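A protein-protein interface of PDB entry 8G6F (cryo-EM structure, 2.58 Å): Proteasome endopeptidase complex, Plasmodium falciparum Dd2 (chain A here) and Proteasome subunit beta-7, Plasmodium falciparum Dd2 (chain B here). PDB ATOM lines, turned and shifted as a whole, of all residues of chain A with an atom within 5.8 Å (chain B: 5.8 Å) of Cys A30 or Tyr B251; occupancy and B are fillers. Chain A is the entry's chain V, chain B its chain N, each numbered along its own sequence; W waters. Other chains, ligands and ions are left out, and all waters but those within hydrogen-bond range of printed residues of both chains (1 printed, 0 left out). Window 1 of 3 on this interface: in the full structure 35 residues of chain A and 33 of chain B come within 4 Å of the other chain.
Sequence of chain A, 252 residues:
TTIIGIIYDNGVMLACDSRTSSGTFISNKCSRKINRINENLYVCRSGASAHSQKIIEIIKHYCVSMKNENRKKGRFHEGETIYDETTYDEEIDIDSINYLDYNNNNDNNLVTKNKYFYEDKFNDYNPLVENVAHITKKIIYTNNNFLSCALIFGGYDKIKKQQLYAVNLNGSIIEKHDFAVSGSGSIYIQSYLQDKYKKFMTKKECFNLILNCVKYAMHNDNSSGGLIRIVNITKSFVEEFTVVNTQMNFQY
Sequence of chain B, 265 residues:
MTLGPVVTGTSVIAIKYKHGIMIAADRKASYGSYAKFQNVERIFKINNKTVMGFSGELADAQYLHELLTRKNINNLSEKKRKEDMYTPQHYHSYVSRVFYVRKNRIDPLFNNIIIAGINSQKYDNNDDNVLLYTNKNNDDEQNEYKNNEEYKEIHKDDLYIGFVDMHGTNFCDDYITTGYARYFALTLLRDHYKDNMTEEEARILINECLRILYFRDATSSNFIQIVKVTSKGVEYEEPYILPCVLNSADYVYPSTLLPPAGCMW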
ATOM      1  N   SER A  18      -4.990  28.772  20.914  1.00  0.00           N
ATOM      2  CA  SER A  18      -6.302  29.391  21.073  1.00  0.00           C
ATOM      3  C   SER A  18      -6.680  29.590  22.534  1.00  0.00           C
ATOM      4  O   SER A  18      -7.865  29.564  22.872  1.00  0.00           O
ATOM      5  CB  SER A  18      -7.382  28.564  20.380  1.00  0.00           C
ATOM      6  OG  SER A  18      -7.583  27.336  21.043  1.00  0.00           O
ATOM      7  N   ARG A  19      -5.709  29.808  23.409  1.00  0.00           N
ATOM      8  CA  ARG A  19      -5.976  29.994  24.829  1.00  0.00           C
ATOM      9  C   ARG A  19      -5.863  31.470  25.182  1.00  0.00           C
ATOM     10  O   ARG A  19      -4.826  32.092  24.939  1.00  0.00           O
ATOM     11  CB  ARG A  19      -5.011  29.172  25.680  1.00  0.00           C
ATOM     12  CG  ARG A  19      -5.100  29.474  27.166  1.00  0.00           C
ATOM     13  CD  ARG A  19      -4.290  28.508  27.993  1.00  0.00           C
ATOM     14  NE  ARG A  19      -4.797  27.146  27.912  1.00  0.00           N
ATOM     15  CZ  ARG A  19      -4.212  26.097  28.469  1.00  0.00           C
ATOM     16  NH1 ARG A  19      -3.087  26.216  29.150  1.00  0.00           N
ATOM     17  NH2 ARG A  19      -4.772  24.900  28.343  1.00  0.00           N
ATOM     18  N   ASN A  28     -11.024  32.097  27.977  1.00  0.00           N
ATOM     19  CA  ASN A  28     -11.506  31.538  26.718  1.00  0.00           C
ATOM     20  C   ASN A  28     -10.685  30.308  26.375  1.00  0.00           C
ATOM     21  O   ASN A  28      -9.464  30.396  26.216  1.00  0.00           O
ATOM     22  CB  ASN A  28     -11.423  32.554  25.579  1.00  0.00           C
ATOM     23  CG  ASN A  28     -12.205  33.812  25.860  1.00  0.00           C
ATOM     24  OD1 ASN A  28     -11.695  34.916  25.693  1.00  0.00           O
ATOM     25  ND2 ASN A  28     -13.452  33.656  26.281  1.00  0.00           N
ATOM     26  N   LYS A  29     -11.359  29.168  26.243  1.00  0.00           N
ATOM     27  CA  LYS A  29     -10.671  27.932  25.896  1.00  0.00           C
ATOM     28  C   LYS A  29     -10.147  27.972  24.469  1.00  0.00           C
ATOM     29  O   LYS A  29      -8.993  27.613  24.211  1.00  0.00           O
ATOM     30  CB  LYS A  29     -11.614  26.748  26.076  1.00  0.00           C
ATOM     31  CG  LYS A  29     -11.660  26.190  27.472  1.00  0.00           C
ATOM     32  CD  LYS A  29     -12.444  24.897  27.512  1.00  0.00           C
ATOM     33  CE  LYS A  29     -13.828  25.066  26.929  1.00  0.00           C
ATOM     34  NZ  LYS A  29     -14.690  23.905  27.234  1.00  0.00           N
ATOM     35  N   CYS A  30     -10.992  28.379  23.516  1.00  0.00           N
ATOM     36  CA  CYS A  30     -10.665  28.330  22.091  1.00  0.00           C
ATOM     37  C   CYS A  30     -10.999  29.678  21.464  1.00  0.00           C
ATOM     38  O   CYS A  30     -12.069  29.862  20.884  1.00  0.00           O
ATOM     39  CB  CYS A  30     -11.418  27.185  21.416  1.00  0.00           C
ATOM     40  SG  CYS A  30     -11.142  25.582  22.194  1.00  0.00           S
ATOM     41  N   SER A  31     -10.060  30.611  21.550  1.00  0.00           N
ATOM     42  CA  SER A  31     -10.219  31.927  20.956  1.00  0.00           C
ATOM     43  C   SER A  31      -9.653  31.937  19.538  1.00  0.00           C
ATOM     44  O   SER A  31      -8.951  31.020  19.112  1.00  0.00           O
ATOM     45  CB  SER A  31      -9.537  32.981  21.824  1.00  0.00           C
ATOM     46  OG  SER A  31      -8.136  32.936  21.673  1.00  0.00           O
ATOM     47  N   ARG A  32      -9.969  32.993  18.801  1.00  0.00           N
ATOM     48  CA  ARG A  32      -9.594  33.117  17.395  1.00  0.00           C
ATOM     49  C   ARG A  32      -8.588  34.253  17.256  1.00  0.00           C
ATOM     50  O   ARG A  32      -8.964  35.425  17.199  1.00  0.00           O
ATOM     51  CB  ARG A  32     -10.833  33.347  16.541  1.00  0.00           C
ATOM     52  CG  ARG A  32     -11.649  32.089  16.342  1.00  0.00           C
ATOM     53  CD  ARG A  32     -13.134  32.351  16.331  1.00  0.00           C
ATOM     54  NE  ARG A  32     -13.893  31.136  16.595  1.00  0.00           N
ATOM     55  CZ  ARG A  32     -14.007  30.123  15.747  1.00  0.00           C
ATOM     56  NH1 ARG A  32     -13.427  30.144  14.561  1.00  0.00           N
ATOM     57  NH2 ARG A  32     -14.725  29.062  16.098  1.00  0.00           N
ATOM     58  N   GLY A 226      -5.383  24.719  24.200  1.00  0.00           N
ATOM     59  CA  GLY A 226      -6.532  24.616  23.326  1.00  0.00           C
ATOM     60  C   GLY A 226      -6.173  23.943  22.014  1.00  0.00           C
ATOM     61  O   GLY A 226      -5.245  23.140  21.930  1.00  0.00           O
ATOM     62  N   LEU A 227      -6.929  24.279  20.977  1.00  0.00           N
ATOM     63  CA  LEU A 227      -6.708  23.721  19.655  1.00  0.00           C
ATOM     64  C   LEU A 227      -5.703  24.584  18.891  1.00  0.00           C
ATOM     65  O   LEU A 227      -5.195  25.584  19.397  1.00  0.00           O
ATOM     66  CB  LEU A 227      -8.032  23.591  18.903  1.00  0.00           C
ATOM     67  CG  LEU A 227      -9.023  24.756  18.956  1.00  0.00           C
ATOM     68  CD1 LEU A 227      -8.529  25.914  18.120  1.00  0.00           C
ATOM     69  CD2 LEU A 227     -10.379  24.300  18.480  1.00  0.00           C
ATOM     70  N   ARG A 229      -5.071  26.620  15.222  1.00  0.00           N
ATOM     71  CA  ARG A 229      -5.682  27.163  14.017  1.00  0.00           C
ATOM     72  C   ARG A 229      -4.589  27.507  13.021  1.00  0.00           C
ATOM     73  O   ARG A 229      -3.608  28.163  13.382  1.00  0.00           O
ATOM     74  CB  ARG A 229      -6.526  28.396  14.338  1.00  0.00           C
ATOM     75  CG  ARG A 229      -7.515  28.183  15.461  1.00  0.00           C
ATOM     76  CD  ARG A 229      -8.552  29.281  15.506  1.00  0.00           C
ATOM     77  NE  ARG A 229      -9.507  29.092  16.591  1.00  0.00           N
ATOM     78  CZ  ARG A 229     -10.603  28.353  16.508  1.00  0.00           C
ATOM     79  NH1 ARG A 229     -10.922  27.708  15.399  1.00  0.00           N
ATOM     80  NH2 ARG A 229     -11.401  28.257  17.565  1.00  0.00           N
ATOM     81  N   THR A 242      -8.316  23.413  11.398  1.00  0.00           N
ATOM     82  CA  THR A 242      -8.314  23.305  12.849  1.00  0.00           C
ATOM     83  C   THR A 242      -7.758  21.943  13.226  1.00  0.00           C
ATOM     84  O   THR A 242      -8.195  20.922  12.687  1.00  0.00           O
ATOM     85  CB  THR A 242      -9.716  23.477  13.437  1.00  0.00           C
ATOM     86  OG1 THR A 242     -10.347  24.623  12.861  1.00  0.00           O
ATOM     87  CG2 THR A 242      -9.643  23.654  14.936  1.00  0.00           C
ATOM     88  N   ARG B 216      -9.883  24.355  32.331  1.00  0.00           N
ATOM     89  CA  ARG B 216     -10.064  25.721  32.810  1.00  0.00           C
ATOM     90  C   ARG B 216      -8.929  26.245  33.677  1.00  0.00           C
ATOM     91  O   ARG B 216      -9.018  27.376  34.159  1.00  0.00           O
ATOM     92  CB  ARG B 216     -11.376  25.825  33.595  1.00  0.00           C
ATOM     93  CG  ARG B 216     -12.626  25.921  32.742  1.00  0.00           C
ATOM     94  CD  ARG B 216     -12.648  27.152  31.859  1.00  0.00           C
ATOM     95  NE  ARG B 216     -13.697  27.063  30.855  1.00  0.00           N
ATOM     96  CZ  ARG B 216     -13.983  28.019  29.984  1.00  0.00           C
ATOM     97  NH1 ARG B 216     -13.303  29.151  29.954  1.00  0.00           N
ATOM     98  NH2 ARG B 216     -14.975  27.831  29.121  1.00  0.00           N
ATOM     99  N   LEU B 246     -12.768  18.462  23.565  1.00  0.00           N
ATOM    100  CA  LEU B 246     -13.638  19.622  23.672  1.00  0.00           C
ATOM    101  C   LEU B 246     -15.099  19.206  23.561  1.00  0.00           C
ATOM    102  O   LEU B 246     -15.443  18.231  22.889  1.00  0.00           O
ATOM    103  CB  LEU B 246     -13.297  20.642  22.591  1.00  0.00           C
ATOM    104  CG  LEU B 246     -11.941  21.319  22.779  1.00  0.00           C
ATOM    105  CD1 LEU B 246     -11.448  21.898  21.470  1.00  0.00           C
ATOM    106  CD2 LEU B 246     -12.025  22.392  23.847  1.00  0.00           C
ATOM    107  N   ASN B 247     -15.965  19.962  24.230  1.00  0.00           N
ATOM    108  CA  ASN B 247     -17.374  19.619  24.342  1.00  0.00           C
ATOM    109  C   ASN B 247     -18.255  20.407  23.383  1.00  0.00           C
ATOM    110  O   ASN B 247     -19.478  20.404  23.544  1.00  0.00           O
ATOM    111  CB  ASN B 247     -17.858  19.827  25.781  1.00  0.00           C
ATOM    112  CG  ASN B 247     -17.395  21.140  26.375  1.00  0.00           C
ATOM    113  OD1 ASN B 247     -16.524  21.809  25.827  1.00  0.00           O
ATOM    114  ND2 ASN B 247     -17.979  21.517  27.502  1.00  0.00           N
ATOM    115  N   SER B 248     -17.669  21.077  22.394  1.00  0.00           N
ATOM    116  CA  SER B 248     -18.447  21.834  21.425  1.00  0.00           C
ATOM    117  C   SER B 248     -17.748  21.808  20.074  1.00  0.00           C
ATOM    118  O   SER B 248     -16.517  21.818  20.004  1.00  0.00           O
ATOM    119  CB  SER B 248     -18.646  23.279  21.884  1.00  0.00           C
ATOM    120  OG  SER B 248     -19.765  23.859  21.247  1.00  0.00           O
ATOM    121  N   ALA B 249     -18.542  21.767  19.007  1.00  0.00           N
ATOM    122  CA  ALA B 249     -18.033  21.899  17.650  1.00  0.00           C
ATOM    123  C   ALA B 249     -17.912  23.350  17.206  1.00  0.00           C
ATOM    124  O   ALA B 249     -17.252  23.625  16.194  1.00  0.00           O
ATOM    125  CB  ALA B 249     -18.938  21.142  16.678  1.00  0.00           C
ATOM    126  N   ASP B 250     -18.529  24.280  17.934  1.00  0.00           N
ATOM    127  CA  ASP B 250     -18.343  25.693  17.640  1.00  0.00           C
ATOM    128  C   ASP B 250     -16.905  26.121  17.879  1.00  0.00           C
ATOM    129  O   ASP B 250     -16.423  27.058  17.233  1.00  0.00           O
ATOM    130  CB  ASP B 250     -19.298  26.530  18.482  1.00  0.00           C
ATOM    131  CG  ASP B 250     -20.742  26.145  18.268  1.00  0.00           C
ATOM    132  OD1 ASP B 250     -21.274  26.421  17.173  1.00  0.00           O
ATOM    133  OD2 ASP B 250     -21.347  25.564  19.191  1.00  0.00           O
ATOM    134  N   TYR B 251     -16.207  25.456  18.798  1.00  0.00           N
ATOM    135  CA  TYR B 251     -14.779  25.702  18.958  1.00  0.00           C
ATOM    136  C   TYR B 251     -14.028  25.383  17.674  1.00  0.00           C
ATOM    137  O   TYR B 251     -13.173  26.156  17.229  1.00  0.00           O
ATOM    138  CB  TYR B 251     -14.227  24.854  20.099  1.00  0.00           C
ATOM    139  CG  TYR B 251     -14.835  25.121  21.448  1.00  0.00           C
ATOM    140  CD1 TYR B 251     -15.082  26.414  21.881  1.00  0.00           C
ATOM    141  CD2 TYR B 251     -15.140  24.076  22.302  1.00  0.00           C
ATOM    142  CE1 TYR B 251     -15.625  26.652  23.117  1.00  0.00           C
ATOM    143  CE2 TYR B 251     -15.684  24.307  23.535  1.00  0.00           C
ATOM    144  CZ  TYR B 251     -15.925  25.594  23.940  1.00  0.00           C
ATOM    145  OH  TYR B 251     -16.471  25.821  25.178  1.00  0.00           O
ATOM    146  N   VAL B 252     -14.339  24.239  17.066  1.00  0.00           N
ATOM    147  CA  VAL B 252     -13.588  23.760  15.916  1.00  0.00           C
ATOM    148  C   VAL B 252     -14.026  24.436  14.626  1.00  0.00           C
ATOM    149  O   VAL B 252     -13.291  24.391  13.634  1.00  0.00           O
ATOM    150  CB  VAL B 252     -13.739  22.235  15.798  1.00  0.00           C
ATOM    151  CG1 VAL B 252     -12.728  21.668  14.831  1.00  0.00           C
ATOM    152  CG2 VAL B 252     -13.589  21.585  17.157  1.00  0.00           C
ATOM    153  N   TYR B 253     -15.197  25.056  14.614  1.00  0.00           N
ATOM    154  CA  TYR B 253     -15.684  25.706  13.409  1.00  0.00           C
ATOM    155  C   TYR B 253     -14.635  26.683  12.875  1.00  0.00           C
ATOM    156  O   TYR B 253     -14.162  27.546  13.627  1.00  0.00           O
ATOM    157  CB  TYR B 253     -16.984  26.445  13.718  1.00  0.00           C
ATOM    158  CG  TYR B 253     -17.801  26.824  12.509  1.00  0.00           C
ATOM    159  CD1 TYR B 253     -18.308  25.857  11.655  1.00  0.00           C
ATOM    160  CD2 TYR B 253     -18.079  28.152  12.233  1.00  0.00           C
ATOM    161  CE1 TYR B 253     -19.061  26.206  10.557  1.00  0.00           C
ATOM    162  CE2 TYR B 253     -18.831  28.508  11.140  1.00  0.00           C
ATOM    163  CZ  TYR B 253     -19.319  27.533  10.305  1.00  0.00           C
ATOM    164  OH  TYR B 253     -20.070  27.896   9.212  1.00  0.00           O
ATOM    165  N   PRO B 254     -14.245  26.586  11.601  1.00  0.00           N
ATOM    166  CA  PRO B 254     -13.229  27.504  11.073  1.00  0.00           C
ATOM    167  C   PRO B 254     -13.664  28.959  11.158  1.00  0.00           C
ATOM    168  O   PRO B 254     -14.841  29.292  11.014  1.00  0.00           O
ATOM    169  CB  PRO B 254     -13.067  27.058   9.616  1.00  0.00           C
ATOM    170  CG  PRO B 254     -13.522  25.662   9.591  1.00  0.00           C
ATOM    171  CD  PRO B 254     -14.594  25.542  10.622  1.00  0.00           C
HETATM  172  O   HOH W   1     -14.397  29.404  26.323  1.00  0.00           O
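OD2 of Asp B250 sits at hydrogen-bond distance from OG of Ser B248, 3.1 Å away.
The side-chain hydroxyl (OG) of Ser A18 sits close to the backbone carbonyl oxygen (O) of Lys A29.
The backbone carbonyl oxygen of Ser A18 sits close to the backbone NH of Cys A30, at 3.4 Å.
The side-chain hydroxyl (OG) of Ser A18 sits at hydrogen-bond distance from the backbone NH (N) of Leu A227, 3.1 Å away.
The guanidinium group of Arg A229 sits at hydrogen-bond distance from the backbone carbonyl oxygen of Ser A31.
Among the printed residues, merely in contact across the chains: Leu A227 with Tyr B251 (3.6 Å), Arg A32 with Pro B254 (3.6 Å), Arg A229 with Tyr B253 (3.7 Å), Cys A30 with Leu B246 (3.7 Å), Lys A29 with Arg B216 (3.7 Å), Cys A30 with Tyr B251 (3.8 Å) and Leu A227 with Leu B246 (3.98 Å).
Along chain B the printed residues that touch a printed residue of chain A span positions 216 to 254.
Hydrophobic or aromatic side chains of chain A within 4 Å of the printed part of chain B: Leu A227.
Along chain A the printed residues that touch a printed residue of chain B span positions 29 to 242.
Among the printed residues, no Asp or Glu carboxylate lies within 4 Å of a Lys or Arg side-chain nitrogen of the other chain.
The side-chain amide oxygen (OD1) of Asn B247 lies within hydrogen-bond range of the side-chain amino group (NZ) of Lys A29 (3.1 Å).
The backbone carbonyl oxygen of Asp B250 lies within hydrogen-bond range of the guanidinium group of Arg A32 (2.9 Å).
OH of Tyr B251 sits close to NZ of Lys A29 (3.3 Å).
The backbone carbonyl oxygen (O) of Tyr B251 lies within hydrogen-bond range of the guanidinium group (NH2) of Arg A32 (3.5 Å).
The backbone carbonyl oxygen (O) of Tyr B251 sits at hydrogen-bond distance from the guanidinium group (NH2) of Arg A229, 2.8 Å away.
The backbone carbonyl oxygen of Val B252 is in hydrogen-bond range of the side-chain hydroxyl of Thr A242, at 3.1 Å.
The backbone carbonyl oxygen (O) of Tyr B253 sits at hydrogen-bond distance from the guanidinium group (NH1) of Arg A32, 2.9 Å away.
Water W1 lies within hydrogen-bond range of the backbone NH of Lys A29 and the guanidinium group of Arg B216.
Of the printed residues of chain B, Lys A29 touches Arg B216 (3.7 Å), Asn B247 (3.1 Å) and Tyr B251 (3.3 Å).
Cys A30 touches just these residues of chain B: Leu B246 and Tyr B251.
Printed residues of chain B within 4 Å of Arg A229: Tyr B251 (2.8 Å) and Tyr B253 (3.7 Å).
Ala B249 touches none of the printed residues of chain A.
Tyr B251 touches just these residues of chain A: Lys A29 (3.3 Å), Cys A30 (3.8 Å), Arg A32 (3.5 Å), Leu A227 (3.6 Å) and Arg A229 (2.8 Å).
Of the printed residues of chain A, Tyr B253 touches Arg A32 and Arg A229.
Of the printed residues of chain A, Pro B254 touches Arg A32 (3.6 Å).
The nearest printed residue of chain B that does not touch Cys A30 is Val B252 (6.0 Å).
The nearest residue of chain A that does not touch Tyr B251 is Thr A242 (4.9 Å).
The nearest printed residue of chain A that does not touch Val B252 is Leu A227 (4.1 Å).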
